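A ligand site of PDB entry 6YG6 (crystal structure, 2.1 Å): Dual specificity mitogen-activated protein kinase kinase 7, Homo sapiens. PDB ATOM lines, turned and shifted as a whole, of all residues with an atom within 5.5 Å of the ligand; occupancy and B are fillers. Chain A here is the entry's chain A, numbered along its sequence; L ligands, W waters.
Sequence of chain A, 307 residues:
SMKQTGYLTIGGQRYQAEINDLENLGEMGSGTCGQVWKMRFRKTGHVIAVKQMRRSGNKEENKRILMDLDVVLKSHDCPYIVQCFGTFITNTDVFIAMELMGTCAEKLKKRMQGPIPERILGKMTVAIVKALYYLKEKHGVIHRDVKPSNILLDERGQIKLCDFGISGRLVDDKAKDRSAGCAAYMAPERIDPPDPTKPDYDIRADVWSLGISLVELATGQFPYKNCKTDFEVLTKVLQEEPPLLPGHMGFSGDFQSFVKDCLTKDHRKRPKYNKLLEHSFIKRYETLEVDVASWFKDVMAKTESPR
Water W1 lies within hydrogen-bond range of N2 of the ligand (3.0 Å) and NZ of Lys 51 (3.1 Å).
N of Met 98 is in hydrogen-bond range of O of Ala 49, 2.7 Å away. The backbone NH of Lys 51 is in hydrogen-bond range of the backbone carbonyl oxygen of Ile 96, at 2.9 Å. The backbone carbonyl oxygen (O) of Leu 161 is in hydrogen-bond range of the backbone NH (N) of Val 82 (3.1 Å). The backbone NH (N) of Val 141 lies within hydrogen-bond range of the backbone carbonyl oxygen (O) of Leu 135, at 3.1 Å. The backbone NH (N) of Phe 164 is in hydrogen-bond range of the side-chain amide oxygen (OD1) of Asn 150 (2.7 Å). The backbone carbonyl oxygen (O) of Val 36 sits at hydrogen-bond distance from the backbone NH (N) of Met 28 (3.0 Å). O of Asn 150 is in hydrogen-bond range of N of Cys 162, at 3.0 Å. O of Cys 162 sits at hydrogen-bond distance from NE2 of His 143.
The backbone carbonyl oxygen of Leu 161 sits close to a fluorine (F3) of the ligand. Residues that only touch the ligand: Met 28, Val 36, Ala 49, Val 50, Lys 51, Asp 68, Val 72, Ile 81, Val 82, Met 98, Glu 99, Leu 100, Gly 102, Lys 107, Val 141, Arg 144, Ser 149, Leu 152, Cys 162 and Phe 164. Hydrophobic or aromatic side chains within 4 Å of the ligand: Met 28, Val 36, Ala 49, Val 72, Ile 81, Val 82, Met 98, Met 101, Val 141, His 143, Leu 152 and Phe 164. Of the 35 residues printed, 26 come within 4 Å of the ligand. The nearest printed residue that does not touch the ligand is Ile 96 (4.02 Å).
A nitrogen (N2) of the ligand lies close to the backbone carbonyl oxygen (O) of Asp 163 (3.4 Å). The backbone carbonyl oxygen of Ile 142 sits close to a nitrogen (N5) of the ligand, at 3.4 Å. A nitrogen (N6) of the ligand sits at hydrogen-bond distance from the backbone carbonyl oxygen (O) of Met 101, 2.8 Å away. An oxygen (O1) of the ligand lies within hydrogen-bond range of the backbone NH (N) of Asp 163, 2.8 Å away. A nitrogen (N5) of the ligand lies close to the backbone carbonyl oxygen of His 143. N of Met 101 sits at hydrogen-bond distance from N3 of the ligand, at 3.0 Å. The side-chain sulfur (SG) of Cys 104 is covalently linked to a carbon (C33) of the ligand, at 1.8 Å.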
ATOM      1  N   MET A  28      13.827   3.657  35.988  1.00  0.00           N
ATOM      2  CA  MET A  28      13.477   2.984  34.744  1.00  0.00           C
ATOM      3  C   MET A  28      14.616   2.853  33.736  1.00  0.00           C
ATOM      4  O   MET A  28      14.594   1.937  32.906  1.00  0.00           O
ATOM      5  CB  MET A  28      12.304   3.695  34.093  1.00  0.00           C
ATOM      6  CG  MET A  28      11.033   3.707  34.911  1.00  0.00           C
ATOM      7  SD  MET A  28       9.665   4.389  33.933  1.00  0.00           S
ATOM      8  CE  MET A  28      10.189   6.097  33.702  1.00  0.00           C
ATOM      9  N   VAL A  36      16.675   8.245  34.963  1.00  0.00           N
ATOM     10  CA  VAL A  36      15.239   8.331  34.740  1.00  0.00           C
ATOM     11  C   VAL A  36      14.457   7.616  35.835  1.00  0.00           C
ATOM     12  O   VAL A  36      14.776   6.472  36.205  1.00  0.00           O
ATOM     13  CB  VAL A  36      14.838   7.729  33.364  1.00  0.00           C
ATOM     14  CG1 VAL A  36      13.327   7.790  33.166  1.00  0.00           C
ATOM     15  CG2 VAL A  36      15.544   8.462  32.234  1.00  0.00           C
ATOM     16  N   ALA A  49       7.090  10.139  33.994  1.00  0.00           N
ATOM     17  CA  ALA A  49       8.483   9.797  33.763  1.00  0.00           C
ATOM     18  C   ALA A  49       9.310  11.055  33.961  1.00  0.00           C
ATOM     19  O   ALA A  49       8.997  12.129  33.378  1.00  0.00           O
ATOM     20  CB  ALA A  49       8.649   9.266  32.360  1.00  0.00           C
ATOM     21  N   VAL A  50      10.353  10.946  34.755  1.00  0.00           N
ATOM     22  CA  VAL A  50      11.209  12.092  35.028  1.00  0.00           C
ATOM     23  C   VAL A  50      12.688  11.758  34.783  1.00  0.00           C
ATOM     24  O   VAL A  50      13.213  10.795  35.330  1.00  0.00           O
ATOM     25  CB  VAL A  50      11.023  12.544  36.480  1.00  0.00           C
ATOM     26  CG1 VAL A  50      11.963  13.710  36.806  1.00  0.00           C
ATOM     27  CG2 VAL A  50       9.565  12.936  36.707  1.00  0.00           C
ATOM     28  N   LYS A  51      13.325  12.541  33.907  1.00  0.00           N
ATOM     29  CA  LYS A  51      14.778  12.441  33.669  1.00  0.00           C
ATOM     30  C   LYS A  51      15.543  13.483  34.530  1.00  0.00           C
ATOM     31  O   LYS A  51      15.280  14.677  34.436  1.00  0.00           O
ATOM     32  CB  LYS A  51      15.131  12.634  32.179  1.00  0.00           C
ATOM     33  CG  LYS A  51      16.578  12.221  31.822  1.00  0.00           C
ATOM     34  CD  LYS A  51      16.969  12.621  30.383  1.00  0.00           C
ATOM     35  CE  LYS A  51      16.258  11.787  29.286  1.00  0.00           C
ATOM     36  NZ  LYS A  51      16.591  12.168  27.856  1.00  0.00           N
ATOM     37  N   ASP A  68      17.016  22.117  22.979  1.00  0.00           N
ATOM     38  CA  ASP A  68      16.421  20.815  22.628  1.00  0.00           C
ATOM     39  C   ASP A  68      15.092  20.587  23.359  1.00  0.00           C
ATOM     40  O   ASP A  68      14.103  20.213  22.757  1.00  0.00           O
ATOM     41  CB  ASP A  68      17.389  19.680  22.966  1.00  0.00           C
ATOM     42  CG  ASP A  68      18.614  19.624  22.052  1.00  0.00           C
ATOM     43  OD1 ASP A  68      18.761  20.474  21.132  1.00  0.00           O
ATOM     44  OD2 ASP A  68      19.426  18.688  22.241  1.00  0.00           O
ATOM     45  N   LEU A  69      15.080  20.843  24.649  1.00  0.00           N
ATOM     46  CA  LEU A  69      13.875  20.638  25.442  1.00  0.00           C
ATOM     47  C   LEU A  69      12.773  21.627  25.086  1.00  0.00           C
ATOM     48  O   LEU A  69      11.604  21.318  25.208  1.00  0.00           O
ATOM     49  CB  LEU A  69      14.177  20.776  26.921  1.00  0.00           C
ATOM     50  CG  LEU A  69      15.209  19.851  27.573  1.00  0.00           C
ATOM     51  CD1 LEU A  69      15.370  20.185  29.055  1.00  0.00           C
ATOM     52  CD2 LEU A  69      14.863  18.383  27.401  1.00  0.00           C
ATOM     53  N   VAL A  71      12.134  22.606  22.167  1.00  0.00           N
ATOM     54  CA  VAL A  71      11.466  22.013  21.029  1.00  0.00           C
ATOM     55  C   VAL A  71      10.383  21.003  21.478  1.00  0.00           C
ATOM     56  O   VAL A  71       9.241  21.095  21.025  1.00  0.00           O
ATOM     57  CB  VAL A  71      12.471  21.328  20.048  1.00  0.00           C
ATOM     58  CG1 VAL A  71      11.713  20.604  18.937  1.00  0.00           C
ATOM     59  CG2 VAL A  71      13.412  22.383  19.459  1.00  0.00           C
ATOM     60  N   VAL A  72      10.739  20.085  22.368  1.00  0.00           N
ATOM     61  CA  VAL A  72       9.776  19.097  22.841  1.00  0.00           C
ATOM     62  C   VAL A  72       8.619  19.727  23.577  1.00  0.00           C
ATOM     63  O   VAL A  72       7.472  19.310  23.400  1.00  0.00           O
ATOM     64  CB  VAL A  72      10.401  18.123  23.828  1.00  0.00           C
ATOM     65  CG1 VAL A  72       9.352  17.059  24.205  1.00  0.00           C
ATOM     66  CG2 VAL A  72      11.635  17.535  23.216  1.00  0.00           C
ATOM     67  N   SER A  75       6.114  20.738  21.137  1.00  0.00           N
ATOM     68  CA  SER A  75       5.736  19.669  20.192  1.00  0.00           C
ATOM     69  C   SER A  75       4.447  18.943  20.626  1.00  0.00           C
ATOM     70  O   SER A  75       4.115  17.888  20.107  1.00  0.00           O
ATOM     71  CB  SER A  75       6.873  18.676  20.022  1.00  0.00           C
ATOM     72  OG  SER A  75       7.940  19.327  19.381  1.00  0.00           O
ATOM     73  N   ILE A  81       5.174  12.484  19.020  1.00  0.00           N
ATOM     74  CA  ILE A  81       6.293  12.889  19.803  1.00  0.00           C
ATOM     75  C   ILE A  81       5.855  12.837  21.249  1.00  0.00           C
ATOM     76  O   ILE A  81       4.807  13.347  21.609  1.00  0.00           O
ATOM     77  CB  ILE A  81       6.776  14.280  19.411  1.00  0.00           C
ATOM     78  CG1 ILE A  81       7.517  14.206  18.067  1.00  0.00           C
ATOM     79  CG2 ILE A  81       7.719  14.871  20.453  1.00  0.00           C
ATOM     80  CD1 ILE A  81       7.626  15.531  17.380  1.00  0.00           C
ATOM     81  N   VAL A  82       6.682  12.202  22.064  1.00  0.00           N
ATOM     82  CA  VAL A  82       6.404  12.077  23.468  1.00  0.00           C
ATOM     83  C   VAL A  82       6.146  13.464  24.088  1.00  0.00           C
ATOM     84  O   VAL A  82       6.865  14.431  23.795  1.00  0.00           O
ATOM     85  CB  VAL A  82       7.518  11.321  24.209  1.00  0.00           C
ATOM     86  CG1 VAL A  82       8.825  12.098  24.220  1.00  0.00           C
ATOM     87  CG2 VAL A  82       7.064  10.963  25.623  1.00  0.00           C
ATOM     88  N   ILE A  96      13.312  16.744  33.972  1.00  0.00           N
ATOM     89  CA  ILE A  96      12.464  16.825  32.820  1.00  0.00           C
ATOM     90  C   ILE A  96      11.300  15.830  32.969  1.00  0.00           C
ATOM     91  O   ILE A  96      11.526  14.631  33.115  1.00  0.00           O
ATOM     92  CB  ILE A  96      13.266  16.488  31.568  1.00  0.00           C
ATOM     93  CG1 ILE A  96      14.567  17.316  31.572  1.00  0.00           C
ATOM     94  CG2 ILE A  96      12.423  16.747  30.316  1.00  0.00           C
ATOM     95  CD1 ILE A  96      15.615  16.810  30.618  1.00  0.00           C
ATOM     96  N   MET A  98       7.828  13.987  31.798  1.00  0.00           N
ATOM     97  CA  MET A  98       7.128  13.547  30.619  1.00  0.00           C
ATOM     98  C   MET A  98       5.937  12.617  30.935  1.00  0.00           C
ATOM     99  O   MET A  98       5.881  12.049  31.996  1.00  0.00           O
ATOM    100  CB  MET A  98       8.074  12.758  29.708  1.00  0.00           C
ATOM    101  CG  MET A  98       9.481  13.322  29.510  1.00  0.00           C
ATOM    102  SD  MET A  98       9.552  14.867  28.566  1.00  0.00           S
ATOM    103  CE  MET A  98       9.180  14.331  26.971  1.00  0.00           C
ATOM    104  N   GLU A  99       4.999  12.483  30.002  1.00  0.00           N
ATOM    105  CA  GLU A  99       4.001  11.402  30.033  1.00  0.00           C
ATOM    106  C   GLU A  99       4.748  10.079  30.046  1.00  0.00           C
ATOM    107  O   GLU A  99       5.681   9.882  29.274  1.00  0.00           O
ATOM    108  CB  GLU A  99       3.067  11.452  28.795  1.00  0.00           C
ATOM    109  CG  GLU A  99       3.721  11.138  27.466  1.00  0.00           C
ATOM    110  CD  GLU A  99       2.755  11.017  26.288  1.00  0.00           C
ATOM    111  OE1 GLU A  99       1.578  10.673  26.463  1.00  0.00           O
ATOM    112  OE2 GLU A  99       3.195  11.275  25.146  1.00  0.00           O
ATOM    113  N   LEU A 100       4.340   9.178  30.896  1.00  0.00           N
ATOM    114  CA  LEU A 100       4.965   7.854  30.947  1.00  0.00           C
ATOM    115  C   LEU A 100       4.545   6.950  29.773  1.00  0.00           C
ATOM    116  O   LEU A 100       3.371   6.669  29.598  1.00  0.00           O
ATOM    117  CB  LEU A 100       4.586   7.191  32.261  1.00  0.00           C
ATOM    118  CG  LEU A 100       5.116   5.790  32.534  1.00  0.00           C
ATOM    119  CD1 LEU A 100       6.633   5.820  32.528  1.00  0.00           C
ATOM    120  CD2 LEU A 100       4.605   5.304  33.885  1.00  0.00           C
ATOM    121  N   MET A 101       5.495   6.502  28.972  1.00  0.00           N
ATOM    122  CA  MET A 101       5.261   5.415  27.994  1.00  0.00           C
ATOM    123  C   MET A 101       5.828   4.120  28.586  1.00  0.00           C
ATOM    124  O   MET A 101       6.920   4.121  29.101  1.00  0.00           O
ATOM    125  CB  MET A 101       5.980   5.699  26.715  1.00  0.00           C
ATOM    126  CG  MET A 101       5.680   7.048  26.137  1.00  0.00           C
ATOM    127  SD  MET A 101       4.106   7.124  25.353  1.00  0.00           S
ATOM    128  CE  MET A 101       4.341   6.156  23.864  1.00  0.00           C
ATOM    129  N   GLY A 102       5.110   3.019  28.471  1.00  0.00           N
ATOM    130  CA  GLY A 102       5.468   1.795  29.138  1.00  0.00           C
ATOM    131  C   GLY A 102       6.848   1.266  28.756  1.00  0.00           C
ATOM    132  O   GLY A 102       7.580   0.780  29.614  1.00  0.00           O
ATOM    133  N   THR A 103       7.201   1.364  27.486  1.00  0.00           N
ATOM    134  CA  THR A 103       8.488   0.813  27.047  1.00  0.00           C
ATOM    135  C   THR A 103       8.974   1.386  25.738  1.00  0.00           C
ATOM    136  O   THR A 103       8.335   2.287  25.170  1.00  0.00           O
ATOM    137  CB  THR A 103       8.452  -0.743  26.993  1.00  0.00           C
ATOM    138  OG1 THR A 103       9.770  -1.224  26.763  1.00  0.00           O
ATOM    139  CG2 THR A 103       7.515  -1.226  25.897  1.00  0.00           C
ATOM    140  N   CYS A 104      10.155   0.933  25.316  1.00  0.00           N
ATOM    141  CA  CYS A 104      10.719   1.313  23.992  1.00  0.00           C
ATOM    142  C   CYS A 104      10.918   0.091  23.109  1.00  0.00           C
ATOM    143  O   CYS A 104      10.904  -1.051  23.578  1.00  0.00           O
ATOM    144  CB  CYS A 104      12.015   2.074  24.144  1.00  0.00           C
ATOM    145  SG  CYS A 104      13.253   1.147  25.091  1.00  0.00           S
ATOM    146  N   GLU A 106      13.481  -1.045  21.678  1.00  0.00           N
ATOM    147  CA  GLU A 106      14.665  -1.830  22.039  1.00  0.00           C
ATOM    148  C   GLU A 106      14.313  -2.911  23.072  1.00  0.00           C
ATOM    149  O   GLU A 106      14.774  -4.035  22.945  1.00  0.00           O
ATOM    150  CB  GLU A 106      15.776  -0.936  22.581  1.00  0.00           C
ATOM    151  CG  GLU A 106      17.090  -1.675  22.845  1.00  0.00           C
ATOM    152  CD  GLU A 106      17.881  -1.154  24.038  1.00  0.00           C
ATOM    153  OE1 GLU A 106      17.479  -0.164  24.714  1.00  0.00           O
ATOM    154  OE2 GLU A 106      18.953  -1.753  24.302  1.00  0.00           O
ATOM    155  N   LYS A 107      13.506  -2.560  24.079  1.00  0.00           N
ATOM    156  CA  LYS A 107      13.180  -3.488  25.161  1.00  0.00           C
ATOM    157  C   LYS A 107      12.137  -4.470  24.697  1.00  0.00           C
ATOM    158  O   LYS A 107      12.141  -5.606  25.150  1.00  0.00           O
ATOM    159  CB  LYS A 107      12.674  -2.770  26.423  1.00  0.00           C
ATOM    160  CG  LYS A 107      13.642  -1.783  27.034  1.00  0.00           C
ATOM    161  CD  LYS A 107      14.449  -2.377  28.169  1.00  0.00           C
ATOM    162  CE  LYS A 107      14.920  -1.271  29.119  1.00  0.00           C
ATOM    163  NZ  LYS A 107      15.871  -1.817  30.129  1.00  0.00           N
ATOM    164  N   LEU A 135       9.264  17.647  13.273  1.00  0.00           N
ATOM    165  CA  LEU A 135      10.436  18.329  13.867  1.00  0.00           C
ATOM    166  C   LEU A 135      11.170  19.196  12.854  1.00  0.00           C
ATOM    167  O   LEU A 135      11.562  20.319  13.160  1.00  0.00           O
ATOM    168  CB  LEU A 135      11.416  17.349  14.485  1.00  0.00           C
ATOM    169  CG  LEU A 135      10.971  16.668  15.779  1.00  0.00           C
ATOM    170  CD1 LEU A 135      12.025  15.702  16.243  1.00  0.00           C
ATOM    171  CD2 LEU A 135      10.677  17.681  16.865  1.00  0.00           C
ATOM    172  N   VAL A 141      14.449  21.327  12.936  1.00  0.00           N
ATOM    173  CA  VAL A 141      15.304  20.525  13.783  1.00  0.00           C
ATOM    174  C   VAL A 141      15.423  19.090  13.255  1.00  0.00           C
ATOM    175  O   VAL A 141      14.466  18.520  12.757  1.00  0.00           O
ATOM    176  CB  VAL A 141      14.737  20.562  15.224  1.00  0.00           C
ATOM    177  CG1 VAL A 141      15.193  19.396  16.058  1.00  0.00           C
ATOM    178  CG2 VAL A 141      15.108  21.876  15.886  1.00  0.00           C
ATOM    179  N   ILE A 142      16.608  18.534  13.413  1.00  0.00           N
ATOM    180  CA  ILE A 142      16.928  17.159  13.050  1.00  0.00           C
ATOM    181  C   ILE A 142      17.068  16.379  14.346  1.00  0.00           C
ATOM    182  O   ILE A 142      17.571  16.903  15.318  1.00  0.00           O
ATOM    183  CB  ILE A 142      18.253  17.150  12.237  1.00  0.00           C
ATOM    184  CG1 ILE A 142      18.031  17.779  10.870  1.00  0.00           C
ATOM    185  CG2 ILE A 142      18.795  15.765  12.047  1.00  0.00           C
ATOM    186  CD1 ILE A 142      19.296  18.373  10.263  1.00  0.00           C
ATOM    187  N   HIS A 143      16.644  15.135  14.380  1.00  0.00           N
ATOM    188  CA  HIS A 143      16.714  14.328  15.599  1.00  0.00           C
ATOM    189  C   HIS A 143      18.142  13.901  15.877  1.00  0.00           C
ATOM    190  O   HIS A 143      18.662  14.161  16.941  1.00  0.00           O
ATOM    191  CB  HIS A 143      15.812  13.105  15.515  1.00  0.00           C
ATOM    192  CG  HIS A 143      15.664  12.367  16.803  1.00  0.00           C
ATOM    193  ND1 HIS A 143      16.596  11.443  17.245  1.00  0.00           N
ATOM    194  CD2 HIS A 143      14.711  12.414  17.765  1.00  0.00           C
ATOM    195  CE1 HIS A 143      16.226  10.968  18.423  1.00  0.00           C
ATOM    196  NE2 HIS A 143      15.066  11.514  18.743  1.00  0.00           N
ATOM    197  N   ARG A 144      18.775  13.270  14.896  1.00  0.00           N
ATOM    198  CA  ARG A 144      20.195  12.806  14.932  1.00  0.00           C
ATOM    199  C   ARG A 144      20.474  11.474  15.660  1.00  0.00           C
ATOM    200  O   ARG A 144      21.608  11.016  15.677  1.00  0.00           O
ATOM    201  CB  ARG A 144      21.157  13.876  15.478  1.00  0.00           C
ATOM    202  CG  ARG A 144      21.038  15.213  14.814  1.00  0.00           C
ATOM    203  CD  ARG A 144      22.000  16.272  15.387  1.00  0.00           C
ATOM    204  NE  ARG A 144      21.677  17.611  14.812  1.00  0.00           N
ATOM    205  CZ  ARG A 144      22.261  18.205  13.752  1.00  0.00           C
ATOM    206  NH1 ARG A 144      21.806  19.410  13.357  1.00  0.00           N
ATOM    207  NH2 ARG A 144      23.275  17.648  13.091  1.00  0.00           N
ATOM    208  N   PRO A 148      16.044   2.093  18.004  1.00  0.00           N
ATOM    209  CA  PRO A 148      14.911   1.510  18.730  1.00  0.00           C
ATOM    210  C   PRO A 148      14.693   1.969  20.174  1.00  0.00           C
ATOM    211  O   PRO A 148      13.545   1.926  20.652  1.00  0.00           O
ATOM    212  CB  PRO A 148      15.208   0.019  18.686  1.00  0.00           C
ATOM    213  CG  PRO A 148      15.925  -0.164  17.363  1.00  0.00           C
ATOM    214  CD  PRO A 148      16.829   1.047  17.287  1.00  0.00           C
ATOM    215  N   SER A 149      15.768   2.383  20.859  1.00  0.00           N
ATOM    216  CA  SER A 149      15.642   2.808  22.223  1.00  0.00           C
ATOM    217  C   SER A 149      14.972   4.193  22.328  1.00  0.00           C
ATOM    218  O   SER A 149      14.552   4.589  23.406  1.00  0.00           O
ATOM    219  CB  SER A 149      17.001   2.788  22.940  1.00  0.00           C
ATOM    220  OG  SER A 149      17.894   3.678  22.305  1.00  0.00           O
ATOM    221  N   ASN A 150      14.846   4.891  21.196  1.00  0.00           N
ATOM    222  CA  ASN A 150      14.178   6.161  21.114  1.00  0.00           C
ATOM    223  C   ASN A 150      12.826   6.091  20.441  1.00  0.00           C
ATOM    224  O   ASN A 150      12.285   7.109  19.997  1.00  0.00           O
ATOM    225  CB  ASN A 150      15.097   7.140  20.393  1.00  0.00           C
ATOM    226  CG  ASN A 150      16.226   7.608  21.269  1.00  0.00           C
ATOM    227  OD1 ASN A 150      16.121   7.604  22.482  1.00  0.00           O
ATOM    228  ND2 ASN A 150      17.333   7.994  20.650  1.00  0.00           N
ATOM    229  N   LEU A 152       9.162   4.903  21.498  1.00  0.00           N
ATOM    230  CA  LEU A 152       8.381   4.506  22.695  1.00  0.00           C
ATOM    231  C   LEU A 152       7.066   3.916  22.264  1.00  0.00           C
ATOM    232  O   LEU A 152       6.509   4.330  21.265  1.00  0.00           O
ATOM    233  CB  LEU A 152       8.110   5.736  23.607  1.00  0.00           C
ATOM    234  CG  LEU A 152       9.363   6.415  24.152  1.00  0.00           C
ATOM    235  CD1 LEU A 152       9.027   7.535  25.122  1.00  0.00           C
ATOM    236  CD2 LEU A 152      10.286   5.394  24.810  1.00  0.00           C
ATOM    237  N   LEU A 161       8.185   9.034  19.064  1.00  0.00           N
ATOM    238  CA  LEU A 161       9.585   9.326  19.030  1.00  0.00           C
ATOM    239  C   LEU A 161       9.946  10.085  20.311  1.00  0.00           C
ATOM    240  O   LEU A 161       9.172  10.907  20.797  1.00  0.00           O
ATOM    241  CB  LEU A 161       9.887  10.258  17.837  1.00  0.00           C
ATOM    242  CG  LEU A 161      11.346  10.647  17.580  1.00  0.00           C
ATOM    243  CD1 LEU A 161      12.157   9.430  17.239  1.00  0.00           C
ATOM    244  CD2 LEU A 161      11.396  11.679  16.489  1.00  0.00           C
ATOM    245  N   CYS A 162      11.107   9.751  20.862  1.00  0.00           N
ATOM    246  CA  CYS A 162      11.644  10.418  22.009  1.00  0.00           C
ATOM    247  C   CYS A 162      13.149  10.585  21.812  1.00  0.00           C
ATOM    248  O   CYS A 162      13.716  10.207  20.775  1.00  0.00           O
ATOM    249  CB  CYS A 162      11.337   9.609  23.256  1.00  0.00           C
ATOM    250  SG  CYS A 162      12.340   8.140  23.540  1.00  0.00           S
ATOM    251  N   ASP A 163      13.794  11.158  22.823  1.00  0.00           N
ATOM    252  CA  ASP A 163      15.221  11.087  22.966  1.00  0.00           C
ATOM    253  C   ASP A 163      15.562  10.658  24.383  1.00  0.00           C
ATOM    254  O   ASP A 163      15.618  11.467  25.301  1.00  0.00           O
ATOM    255  CB  ASP A 163      15.877  12.406  22.597  1.00  0.00           C
ATOM    256  CG  ASP A 163      17.386  12.291  22.502  1.00  0.00           C
ATOM    257  OD1 ASP A 163      17.967  11.294  22.973  1.00  0.00           O
ATOM    258  OD2 ASP A 163      18.008  13.210  21.944  1.00  0.00           O
ATOM    259  N   PHE A 164      15.799   9.378  24.537  1.00  0.00           N
ATOM    260  CA  PHE A 164      16.004   8.779  25.836  1.00  0.00           C
ATOM    261  C   PHE A 164      17.403   8.973  26.367  1.00  0.00           C
ATOM    262  O   PHE A 164      17.603   8.836  27.566  1.00  0.00           O
ATOM    263  CB  PHE A 164      15.734   7.290  25.749  1.00  0.00           C
ATOM    264  CG  PHE A 164      15.507   6.618  27.056  1.00  0.00           C
ATOM    265  CD1 PHE A 164      14.341   6.865  27.776  1.00  0.00           C
ATOM    266  CD2 PHE A 164      16.417   5.663  27.531  1.00  0.00           C
ATOM    267  CE1 PHE A 164      14.115   6.213  28.983  1.00  0.00           C
ATOM    268  CE2 PHE A 164      16.196   5.018  28.726  1.00  0.00           C
ATOM    269  CZ  PHE A 164      15.034   5.288  29.453  1.00  0.00           C
HETATM  270  C1  LIG L   1      14.241  16.651  20.532  1.00  0.00           C
HETATM  271  C2  LIG L   1      13.952  15.963  21.857  1.00  0.00           C
HETATM  272  C3  LIG L   1      12.977  14.971  21.967  1.00  0.00           C
HETATM  273  N1  LIG L   1      15.668  16.805  20.270  1.00  0.00           N
HETATM  274  C4  LIG L   1      12.087  14.556  20.817  1.00  0.00           C
HETATM  275  C5  LIG L   1      14.677  16.335  22.988  1.00  0.00           C
HETATM  276  N2  LIG L   1      13.415  14.041  25.567  1.00  0.00           N
HETATM  277  C6  LIG L   1      14.458  15.730  24.207  1.00  0.00           C
HETATM  278  C7  LIG L   1      13.501  14.732  24.330  1.00  0.00           C
HETATM  279  C8  LIG L   1      12.762  14.370  23.200  1.00  0.00           C
HETATM  280  C9  LIG L   1      12.724  12.896  25.826  1.00  0.00           C
HETATM  281  N3  LIG L   1       8.315   7.576  28.950  1.00  0.00           N
HETATM  282  C10 LIG L   1      12.680  12.437  27.251  1.00  0.00           C
HETATM  283  C11 LIG L   1      12.769  13.243  28.378  1.00  0.00           C
HETATM  284  C12 LIG L   1      12.628  12.698  29.646  1.00  0.00           C
HETATM  285  N4  LIG L   1      10.695   7.353  29.126  1.00  0.00           N
HETATM  286  O1  LIG L   1      12.220  12.211  24.940  1.00  0.00           O
HETATM  287  F1  LIG L   1      12.743  13.895  19.871  1.00  0.00           F
HETATM  288  F2  LIG L   1      11.503  15.588  20.227  1.00  0.00           F
HETATM  289  F3  LIG L   1      11.106  13.745  21.189  1.00  0.00           F
HETATM  290  C13 LIG L   1      16.332  15.516  20.072  1.00  0.00           C
HETATM  291  C14 LIG L   1      17.819  15.715  19.878  1.00  0.00           C
HETATM  292  N5  LIG L   1      18.086  16.581  18.710  1.00  0.00           N
HETATM  293  C15 LIG L   1      19.556  16.838  18.596  1.00  0.00           C
HETATM  294  C16 LIG L   1      19.942  18.036  17.723  1.00  0.00           C
HETATM  295  C17 LIG L   1      15.880  17.609  19.080  1.00  0.00           C
HETATM  296  C18 LIG L   1      17.352  17.850  18.853  1.00  0.00           C
HETATM  297  C19 LIG L   1      12.464  11.074  27.415  1.00  0.00           C
HETATM  298  C20 LIG L   1      12.301  10.538  28.680  1.00  0.00           C
HETATM  299  C21 LIG L   1      12.358  11.348  29.823  1.00  0.00           C
HETATM  300  C22 LIG L   1      12.045  10.798  31.186  1.00  0.00           C
HETATM  301  O2  LIG L   1      12.063   9.179  28.795  1.00  0.00           O
HETATM  302  C23 LIG L   1      10.806   8.631  28.775  1.00  0.00           C
HETATM  303  C24 LIG L   1       9.440   6.879  29.168  1.00  0.00           C
HETATM  304  C25 LIG L   1       8.492   8.858  28.576  1.00  0.00           C
HETATM  305  C26 LIG L   1       9.727   9.455  28.461  1.00  0.00           C
HETATM  306  N6  LIG L   1       9.301   5.563  29.408  1.00  0.00           N
HETATM  307  C27 LIG L   1      10.433   4.672  29.642  1.00  0.00           C
HETATM  308  C28 LIG L   1      10.054   3.323  30.151  1.00  0.00           C
HETATM  309  C29 LIG L   1      11.303   2.498  29.872  1.00  0.00           C
HETATM  310  N7  LIG L   1      11.887   3.159  28.696  1.00  0.00           N
HETATM  311  C30 LIG L   1      11.110   4.330  28.323  1.00  0.00           C
HETATM  312  C31 LIG L   1      13.005   2.636  28.131  1.00  0.00           C
HETATM  313  O3  LIG L   1      13.559   1.659  28.604  1.00  0.00           O
HETATM  314  C32 LIG L   1      13.545   3.294  26.884  1.00  0.00           C
HETATM  315  C33 LIG L   1      14.322   2.330  25.970  1.00  0.00           C
HETATM  316  O   HOH W   1      15.514  15.079  27.482  1.00  0.00           O
